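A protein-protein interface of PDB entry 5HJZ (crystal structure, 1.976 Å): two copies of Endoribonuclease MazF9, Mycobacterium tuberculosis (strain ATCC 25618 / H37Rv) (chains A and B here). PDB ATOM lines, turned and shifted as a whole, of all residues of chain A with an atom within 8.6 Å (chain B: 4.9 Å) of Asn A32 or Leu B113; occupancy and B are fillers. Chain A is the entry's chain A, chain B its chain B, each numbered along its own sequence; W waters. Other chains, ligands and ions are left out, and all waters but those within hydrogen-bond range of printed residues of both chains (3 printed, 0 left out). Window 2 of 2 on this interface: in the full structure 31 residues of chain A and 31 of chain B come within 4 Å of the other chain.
CB of Asp B116 touches NE of Arg A5, at 3.8 Å. His B114 touches Ser A31 (O to CA, 3.7 Å). Asn A32 touches Leu B113. Thr A48 touches Leu B115. CB of Leu B111 touches CD1 of Leu A117 (3.9 Å). Leu A117 touches Lys B112 (O to CE, 3.9 Å).
Water W2 bridges the guanidinium group (NH1) of Arg A5 (2.7 Å) and the side-chain carboxylate (OD2) of Asp B116 (3.4 Å). Water W1 lies within hydrogen-bond range of O of Val A46 (2.8 Å), OG1 of Thr A48 (3.1 Å) and NE2 of His B114 (3.5 Å). Water W3 bridges the backbone NH (N) of Asp A33 and the side-chain carboxylate (OD2) of Asp B116.
Of the printed residues of chain B, Val A30 touches Leu B115. Printed residues of chain A within 4 Å of Leu B111: Leu A117. Of the printed residues of chain A, Lys B112 touches Leu A117 (3.9 Å). The nearest residue of chain A that does not touch Leu B113 is Ser A31 (6.7 Å).
The guanidinium group (NH2) of Arg A5 sits at hydrogen-bond distance from the backbone carbonyl oxygen (O) of Leu B115 (2.8 Å). The backbone carbonyl oxygen of His B114 lies within hydrogen-bond range of the side-chain amide nitrogen of Asn A32, 2.9 Å away. A ring nitrogen (NE2) of His B114 is in hydrogen-bond range of the side-chain hydroxyl (OG1) of Thr A48 (2.8 Å). The backbone carbonyl oxygen (O) of Leu B115 sits close to the backbone carbonyl oxygen (O) of Val A30, at 3.4 Å.
The backbone NH (N) of Arg A5 sits at hydrogen-bond distance from the side-chain carboxylate (OD1) of Asp A33, 2.9 Å away. N of Val A30 is in hydrogen-bond range of O of Thr A48 (2.8 Å). The side-chain hydroxyl (OG) of Ser A31 sits at hydrogen-bond distance from the side-chain amide oxygen (OD1) of Asn A36 (2.5 Å). The backbone NH of Arg A34 lies within hydrogen-bond range of the side-chain amide oxygen of Asn A32, 3.0 Å away. OD1 of Asn A32 is in hydrogen-bond range of N of Ala A35 (2.9 Å). O of Asn A32 sits at hydrogen-bond distance from ND2 of Asn A36, at 3.0 Å.
Hydrophobic or aromatic side chains of chain B within 4 Å of the printed part of chain A: Leu B111, His B114 and Leu B115. Of the 19 printed residues of chain A, 6 touch a printed residue of chain B. Among the printed residues, no Asp or Glu carboxylate lies within 4 Å of a Lys or Arg side-chain nitrogen of the other chain.
No position is printed for both chains. Of the 10 pairs that touch across the chains among the printed residues, none has its exchanged pair printed and touching as well.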
ATOM      1  N   MET A   3     -24.849  19.963  -0.948  1.00  0.00           N
ATOM      2  CA  MET A   3     -24.067  20.983  -1.634  1.00  0.00           C
ATOM      3  C   MET A   3     -24.790  21.448  -2.893  1.00  0.00           C
ATOM      4  O   MET A   3     -25.586  20.708  -3.474  1.00  0.00           O
ATOM      5  CB  MET A   3     -22.671  20.457  -1.977  1.00  0.00           C
ATOM      6  CG  MET A   3     -22.658  19.394  -3.058  1.00  0.00           C
ATOM      7  SD  MET A   3     -23.703  17.973  -2.681  1.00  0.00           S
ATOM      8  CE  MET A   3     -22.904  17.326  -1.215  1.00  0.00           C
ATOM      9  N   ARG A   4     -24.514  22.680  -3.304  1.00  0.00           N
ATOM     10  CA  ARG A   4     -25.197  23.277  -4.444  1.00  0.00           C
ATOM     11  C   ARG A   4     -24.201  23.893  -5.413  1.00  0.00           C
ATOM     12  O   ARG A   4     -23.118  24.315  -5.010  1.00  0.00           O
ATOM     13  CB  ARG A   4     -26.189  24.339  -3.977  1.00  0.00           C
ATOM     14  CG  ARG A   4     -27.145  23.865  -2.901  1.00  0.00           C
ATOM     15  CD  ARG A   4     -28.133  24.953  -2.535  1.00  0.00           C
ATOM     16  NE  ARG A   4     -29.436  24.390  -2.196  1.00  0.00           N
ATOM     17  CZ  ARG A   4     -30.330  23.998  -3.098  1.00  0.00           C
ATOM     18  NH1 ARG A   4     -30.060  24.104  -4.392  1.00  0.00           N
ATOM     19  NH2 ARG A   4     -31.492  23.494  -2.707  1.00  0.00           N
ATOM     20  N   ARG A   5     -24.574  23.950  -6.687  1.00  0.00           N
ATOM     21  CA  ARG A   5     -23.717  24.543  -7.707  1.00  0.00           C
ATOM     22  C   ARG A   5     -23.470  26.015  -7.395  1.00  0.00           C
ATOM     23  O   ARG A   5     -24.409  26.769  -7.141  1.00  0.00           O
ATOM     24  CB  ARG A   5     -24.341  24.385  -9.095  1.00  0.00           C
ATOM     25  CG  ARG A   5     -23.375  24.645 -10.239  1.00  0.00           C
ATOM     26  CD  ARG A   5     -23.990  24.281 -11.581  1.00  0.00           C
ATOM     27  NE  ARG A   5     -22.999  24.304 -12.653  1.00  0.00           N
ATOM     28  CZ  ARG A   5     -22.645  25.397 -13.322  1.00  0.00           C
ATOM     29  NH1 ARG A   5     -23.202  26.565 -13.029  1.00  0.00           N
ATOM     30  NH2 ARG A   5     -21.732  25.324 -14.281  1.00  0.00           N
ATOM     31  N   GLY A   6     -22.203  26.414  -7.400  1.00  0.00           N
ATOM     32  CA  GLY A   6     -21.840  27.779  -7.070  1.00  0.00           C
ATOM     33  C   GLY A   6     -21.271  27.906  -5.669  1.00  0.00           C
ATOM     34  O   GLY A   6     -20.552  28.857  -5.368  1.00  0.00           O
ATOM     35  N   VAL A  29     -18.491  24.063  -6.587  1.00  0.00           N
ATOM     36  CA  VAL A  29     -19.375  23.034  -7.124  1.00  0.00           C
ATOM     37  C   VAL A  29     -19.913  23.450  -8.489  1.00  0.00           C
ATOM     38  O   VAL A  29     -20.478  24.535  -8.631  1.00  0.00           O
ATOM     39  CB  VAL A  29     -20.559  22.751  -6.179  1.00  0.00           C
ATOM     40  CG1 VAL A  29     -21.462  21.675  -6.763  1.00  0.00           C
ATOM     41  CG2 VAL A  29     -20.060  22.349  -4.796  1.00  0.00           C
ATOM     42  N   VAL A  30     -19.740  22.590  -9.491  1.00  0.00           N
ATOM     43  CA  VAL A  30     -20.160  22.922 -10.850  1.00  0.00           C
ATOM     44  C   VAL A  30     -21.083  21.870 -11.466  1.00  0.00           C
ATOM     45  O   VAL A  30     -21.648  22.087 -12.538  1.00  0.00           O
ATOM     46  CB  VAL A  30     -18.948  23.117 -11.782  1.00  0.00           C
ATOM     47  CG1 VAL A  30     -18.126  24.315 -11.333  1.00  0.00           C
ATOM     48  CG2 VAL A  30     -18.098  21.859 -11.819  1.00  0.00           C
ATOM     49  N   SER A  31     -21.226  20.729 -10.799  1.00  0.00           N
ATOM     50  CA  SER A  31     -22.204  19.733 -11.221  1.00  0.00           C
ATOM     51  C   SER A  31     -23.608  20.272 -10.960  1.00  0.00           C
ATOM     52  O   SER A  31     -23.811  21.040 -10.019  1.00  0.00           O
ATOM     53  CB  SER A  31     -21.986  18.406 -10.491  1.00  0.00           C
ATOM     54  OG  SER A  31     -22.015  18.585  -9.086  1.00  0.00           O
ATOM     55  N   ASN A  32     -24.569  19.881 -11.794  1.00  0.00           N
ATOM     56  CA  ASN A  32     -25.934  20.388 -11.673  1.00  0.00           C
ATOM     57  C   ASN A  32     -26.579  19.951 -10.362  1.00  0.00           C
ATOM     58  O   ASN A  32     -26.155  18.974  -9.745  1.00  0.00           O
ATOM     59  CB  ASN A  32     -26.791  19.937 -12.859  1.00  0.00           C
ATOM     60  CG  ASN A  32     -27.091  18.452 -12.834  1.00  0.00           C
ATOM     61  OD1 ASN A  32     -28.034  18.009 -12.178  1.00  0.00           O
ATOM     62  ND2 ASN A  32     -26.292  17.672 -13.557  1.00  0.00           N
ATOM     63  N   ASP A  33     -27.610  20.675  -9.945  1.00  0.00           N
ATOM     64  CA  ASP A  33     -28.195  20.466  -8.626  1.00  0.00           C
ATOM     65  C   ASP A  33     -29.045  19.200  -8.523  1.00  0.00           C
ATOM     66  O   ASP A  33     -29.275  18.702  -7.424  1.00  0.00           O
ATOM     67  CB  ASP A  33     -29.021  21.687  -8.222  1.00  0.00           C
ATOM     68  CG  ASP A  33     -28.156  22.837  -7.747  1.00  0.00           C
ATOM     69  OD1 ASP A  33     -27.019  22.573  -7.299  1.00  0.00           O
ATOM     70  OD2 ASP A  33     -28.606  24.000  -7.817  1.00  0.00           O
ATOM     71  N   ARG A  34     -29.501  18.670  -9.654  1.00  0.00           N
ATOM     72  CA  ARG A  34     -30.246  17.414  -9.633  1.00  0.00           C
ATOM     73  C   ARG A  34     -29.315  16.270  -9.243  1.00  0.00           C
ATOM     74  O   ARG A  34     -29.682  15.402  -8.450  1.00  0.00           O
ATOM     75  CB  ARG A  34     -30.907  17.138 -10.988  1.00  0.00           C
ATOM     76  CG  ARG A  34     -31.765  15.874 -11.025  1.00  0.00           C
ATOM     77  CD  ARG A  34     -32.831  15.960 -12.112  1.00  0.00           C
ATOM     78  NE  ARG A  34     -33.458  14.668 -12.391  1.00  0.00           N
ATOM     79  CZ  ARG A  34     -34.592  14.244 -11.840  1.00  0.00           C
ATOM     80  NH1 ARG A  34     -35.241  15.008 -10.971  1.00  0.00           N
ATOM     81  NH2 ARG A  34     -35.080  13.053 -12.161  1.00  0.00           N
ATOM     82  N   ALA A  35     -28.106  16.282  -9.796  1.00  0.00           N
ATOM     83  CA  ALA A  35     -27.095  15.293  -9.440  1.00  0.00           C
ATOM     84  C   ALA A  35     -26.631  15.500  -8.002  1.00  0.00           C
ATOM     85  O   ALA A  35     -26.433  14.539  -7.257  1.00  0.00           O
ATOM     86  CB  ALA A  35     -25.915  15.366 -10.398  1.00  0.00           C
ATOM     87  N   ASN A  36     -26.462  16.763  -7.619  1.00  0.00           N
ATOM     88  CA  ASN A  36     -26.061  17.102  -6.260  1.00  0.00           C
ATOM     89  C   ASN A  36     -27.115  16.663  -5.248  1.00  0.00           C
ATOM     90  O   ASN A  36     -26.787  16.124  -4.192  1.00  0.00           O
ATOM     91  CB  ASN A  36     -25.802  18.606  -6.135  1.00  0.00           C
ATOM     92  CG  ASN A  36     -24.675  19.081  -7.035  1.00  0.00           C
ATOM     93  OD1 ASN A  36     -23.748  18.330  -7.338  1.00  0.00           O
ATOM     94  ND2 ASN A  36     -24.750  20.336  -7.464  1.00  0.00           N
ATOM     95  N   ALA A  37     -28.381  16.892  -5.585  1.00  0.00           N
ATOM     96  CA  ALA A  37     -29.489  16.490  -4.726  1.00  0.00           C
ATOM     97  C   ALA A  37     -29.593  14.972  -4.627  1.00  0.00           C
ATOM     98  O   ALA A  37     -30.002  14.443  -3.598  1.00  0.00           O
ATOM     99  CB  ALA A  37     -30.798  17.073  -5.235  1.00  0.00           C
ATOM    100  N   THR A  38     -29.222  14.278  -5.698  1.00  0.00           N
ATOM    101  CA  THR A  38     -29.286  12.820  -5.728  1.00  0.00           C
ATOM    102  C   THR A  38     -28.145  12.198  -4.918  1.00  0.00           C
ATOM    103  O   THR A  38     -28.319  11.157  -4.282  1.00  0.00           O
ATOM    104  CB  THR A  38     -29.250  12.292  -7.176  1.00  0.00           C
ATOM    105  OG1 THR A  38     -30.413  12.748  -7.877  1.00  0.00           O
ATOM    106  CG2 THR A  38     -29.223  10.770  -7.202  1.00  0.00           C
ATOM    107  N   ALA A  39     -26.995  12.864  -4.908  1.00  0.00           N
ATOM    108  CA  ALA A  39     -25.823  12.355  -4.200  1.00  0.00           C
ATOM    109  C   ALA A  39     -25.940  12.487  -2.679  1.00  0.00           C
ATOM    110  O   ALA A  39     -25.403  11.664  -1.938  1.00  0.00           O
ATOM    111  CB  ALA A  39     -24.571  13.068  -4.690  1.00  0.00           C
ATOM    112  N   VAL A  46     -21.104  10.916  -6.993  1.00  0.00           N
ATOM    113  CA  VAL A  46     -20.081  11.951  -6.961  1.00  0.00           C
ATOM    114  C   VAL A  46     -20.636  13.309  -7.365  1.00  0.00           C
ATOM    115  O   VAL A  46     -21.674  13.401  -8.021  1.00  0.00           O
ATOM    116  CB  VAL A  46     -18.893  11.603  -7.887  1.00  0.00           C
ATOM    117  CG1 VAL A  46     -18.137  10.391  -7.358  1.00  0.00           C
ATOM    118  CG2 VAL A  46     -19.380  11.360  -9.303  1.00  0.00           C
ATOM    119  N   ILE A  47     -19.942  14.362  -6.951  1.00  0.00           N
ATOM    120  CA  ILE A  47     -20.234  15.707  -7.420  1.00  0.00           C
ATOM    121  C   ILE A  47     -18.988  16.252  -8.101  1.00  0.00           C
ATOM    122  O   ILE A  47     -17.884  15.761  -7.869  1.00  0.00           O
ATOM    123  CB  ILE A  47     -20.658  16.646  -6.277  1.00  0.00           C
ATOM    124  CG1 ILE A  47     -19.486  16.881  -5.325  1.00  0.00           C
ATOM    125  CG2 ILE A  47     -21.864  16.077  -5.539  1.00  0.00           C
ATOM    126  CD1 ILE A  47     -19.645  18.101  -4.451  1.00  0.00           C
ATOM    127  N   THR A  48     -19.163  17.261  -8.943  1.00  0.00           N
ATOM    128  CA  THR A  48     -18.046  17.792  -9.712  1.00  0.00           C
ATOM    129  C   THR A  48     -17.677  19.190  -9.235  1.00  0.00           C
ATOM    130  O   THR A  48     -18.538  20.060  -9.111  1.00  0.00           O
ATOM    131  CB  THR A  48     -18.370  17.820 -11.213  1.00  0.00           C
ATOM    132  OG1 THR A  48     -18.753  16.509 -11.641  1.00  0.00           O
ATOM    133  CG2 THR A  48     -17.158  18.263 -12.007  1.00  0.00           C
ATOM    134  N   LEU A 117     -16.563  23.178 -25.442  1.00  0.00           N
ATOM    135  CA  LEU A 117     -18.012  23.104 -25.565  1.00  0.00           C
ATOM    136  C   LEU A 117     -18.574  24.414 -26.106  1.00  0.00           C
ATOM    137  O   LEU A 117     -19.631  24.434 -26.734  1.00  0.00           O
ATOM    138  CB  LEU A 117     -18.651  22.771 -24.216  1.00  0.00           C
ATOM    139  CG  LEU A 117     -18.243  21.449 -23.560  1.00  0.00           C
ATOM    140  CD1 LEU A 117     -18.912  21.296 -22.200  1.00  0.00           C
ATOM    141  CD2 LEU A 117     -18.580  20.273 -24.462  1.00  0.00           C
ATOM    142  N   PRO B  61     -29.007  10.426 -19.522  1.00  0.00           N
ATOM    143  CA  PRO B  61     -28.764  11.523 -20.467  1.00  0.00           C
ATOM    144  C   PRO B  61     -27.361  12.120 -20.357  1.00  0.00           C
ATOM    145  O   PRO B  61     -26.870  12.709 -21.320  1.00  0.00           O
ATOM    146  CB  PRO B  61     -29.823  12.558 -20.077  1.00  0.00           C
ATOM    147  CG  PRO B  61     -30.929  11.753 -19.507  1.00  0.00           C
ATOM    148  CD  PRO B  61     -30.268  10.616 -18.780  1.00  0.00           C
ATOM    149  N   GLU B 109     -22.818  16.993 -25.546  1.00  0.00           N
ATOM    150  CA  GLU B 109     -24.159  17.253 -25.039  1.00  0.00           C
ATOM    151  C   GLU B 109     -24.325  16.696 -23.631  1.00  0.00           C
ATOM    152  O   GLU B 109     -24.981  17.304 -22.787  1.00  0.00           O
ATOM    153  CB  GLU B 109     -25.203  16.655 -25.978  1.00  0.00           C
ATOM    154  CG  GLU B 109     -25.248  17.320 -27.346  1.00  0.00           C
ATOM    155  CD  GLU B 109     -25.924  16.458 -28.394  1.00  0.00           C
ATOM    156  OE1 GLU B 109     -25.852  15.216 -28.285  1.00  0.00           O
ATOM    157  OE2 GLU B 109     -26.526  17.021 -29.333  1.00  0.00           O
ATOM    158  N   ALA B 110     -23.718  15.539 -23.381  1.00  0.00           N
ATOM    159  CA  ALA B 110     -23.761  14.927 -22.059  1.00  0.00           C
ATOM    160  C   ALA B 110     -22.990  15.769 -21.046  1.00  0.00           C
ATOM    161  O   ALA B 110     -23.372  15.856 -19.880  1.00  0.00           O
ATOM    162  CB  ALA B 110     -23.204  13.513 -22.110  1.00  0.00           C
ATOM    163  N   LEU B 111     -21.904  16.386 -21.500  1.00  0.00           N
ATOM    164  CA  LEU B 111     -21.104  17.257 -20.646  1.00  0.00           C
ATOM    165  C   LEU B 111     -21.855  18.547 -20.317  1.00  0.00           C
ATOM    166  O   LEU B 111     -21.807  19.033 -19.184  1.00  0.00           O
ATOM    167  CB  LEU B 111     -19.764  17.578 -21.312  1.00  0.00           C
ATOM    168  CG  LEU B 111     -18.724  16.454 -21.305  1.00  0.00           C
ATOM    169  CD1 LEU B 111     -17.537  16.804 -22.190  1.00  0.00           C
ATOM    170  CD2 LEU B 111     -18.267  16.161 -19.886  1.00  0.00           C
ATOM    171  N   LYS B 112     -22.548  19.097 -21.309  1.00  0.00           N
ATOM    172  CA  LYS B 112     -23.332  20.308 -21.104  1.00  0.00           C
ATOM    173  C   LYS B 112     -24.441  20.071 -20.084  1.00  0.00           C
ATOM    174  O   LYS B 112     -24.687  20.907 -19.213  1.00  0.00           O
ATOM    175  CB  LYS B 112     -23.935  20.799 -22.421  1.00  0.00           C
ATOM    176  CG  LYS B 112     -22.931  21.338 -23.423  1.00  0.00           C
ATOM    177  CD  LYS B 112     -23.650  21.842 -24.665  1.00  0.00           C
ATOM    178  CE  LYS B 112     -22.683  22.174 -25.786  1.00  0.00           C
ATOM    179  NZ  LYS B 112     -23.406  22.657 -26.997  1.00  0.00           N
ATOM    180  N   LEU B 113     -25.105  18.926 -20.198  1.00  0.00           N
ATOM    181  CA  LEU B 113     -26.197  18.588 -19.295  1.00  0.00           C
ATOM    182  C   LEU B 113     -25.706  18.392 -17.863  1.00  0.00           C
ATOM    183  O   LEU B 113     -26.310  18.905 -16.923  1.00  0.00           O
ATOM    184  CB  LEU B 113     -26.926  17.331 -19.779  1.00  0.00           C
ATOM    185  CG  LEU B 113     -27.759  17.484 -21.055  1.00  0.00           C
ATOM    186  CD1 LEU B 113     -28.497  16.193 -21.379  1.00  0.00           C
ATOM    187  CD2 LEU B 113     -28.736  18.644 -20.928  1.00  0.00           C
ATOM    188  N   HIS B 114     -24.608  17.659 -17.700  1.00  0.00           N
ATOM    189  CA  HIS B 114     -24.085  17.372 -16.367  1.00  0.00           C
ATOM    190  C   HIS B 114     -23.585  18.626 -15.654  1.00  0.00           C
ATOM    191  O   HIS B 114     -23.787  18.787 -14.450  1.00  0.00           O
ATOM    192  CB  HIS B 114     -22.952  16.345 -16.438  1.00  0.00           C
ATOM    193  CG  HIS B 114     -22.269  16.119 -15.125  1.00  0.00           C
ATOM    194  ND1 HIS B 114     -22.909  15.559 -14.040  1.00  0.00           N
ATOM    195  CD2 HIS B 114     -21.006  16.391 -14.718  1.00  0.00           C
ATOM    196  CE1 HIS B 114     -22.069  15.491 -13.023  1.00  0.00           C
ATOM    197  NE2 HIS B 114     -20.907  15.987 -13.408  1.00  0.00           N
ATOM    198  N   LEU B 115     -22.938  19.512 -16.403  1.00  0.00           N
ATOM    199  CA  LEU B 115     -22.304  20.690 -15.822  1.00  0.00           C
ATOM    200  C   LEU B 115     -23.159  21.947 -15.946  1.00  0.00           C
ATOM    201  O   LEU B 115     -22.688  23.050 -15.667  1.00  0.00           O
ATOM    202  CB  LEU B 115     -20.942  20.923 -16.478  1.00  0.00           C
ATOM    203  CG  LEU B 115     -19.915  19.820 -16.215  1.00  0.00           C
ATOM    204  CD1 LEU B 115     -18.718  19.966 -17.134  1.00  0.00           C
ATOM    205  CD2 LEU B 115     -19.477  19.837 -14.758  1.00  0.00           C
ATOM    206  N   ASP B 116     -24.411  21.769 -16.366  1.00  0.00           N
ATOM    207  CA  ASP B 116     -25.364  22.871 -16.492  1.00  0.00           C
ATOM    208  C   ASP B 116     -24.821  23.977 -17.396  1.00  0.00           C
ATOM    209  O   ASP B 116     -24.839  25.154 -17.036  1.00  0.00           O
ATOM    210  CB  ASP B 116     -25.713  23.430 -15.107  1.00  0.00           C
ATOM    211  CG  ASP B 116     -27.008  24.218 -15.102  1.00  0.00           C
ATOM    212  OD1 ASP B 116     -27.810  24.054 -16.044  1.00  0.00           O
ATOM    213  OD2 ASP B 116     -27.225  24.995 -14.148  1.00  0.00           O
HETATM  214  O   HOH W   1     -20.495  14.289 -10.423  1.00  0.00           O
HETATM  215  O   HOH W   2     -25.590  26.905 -11.849  1.00  0.00           O
HETATM  216  O   HOH W   3     -28.176  22.998 -11.676  1.00  0.00           O
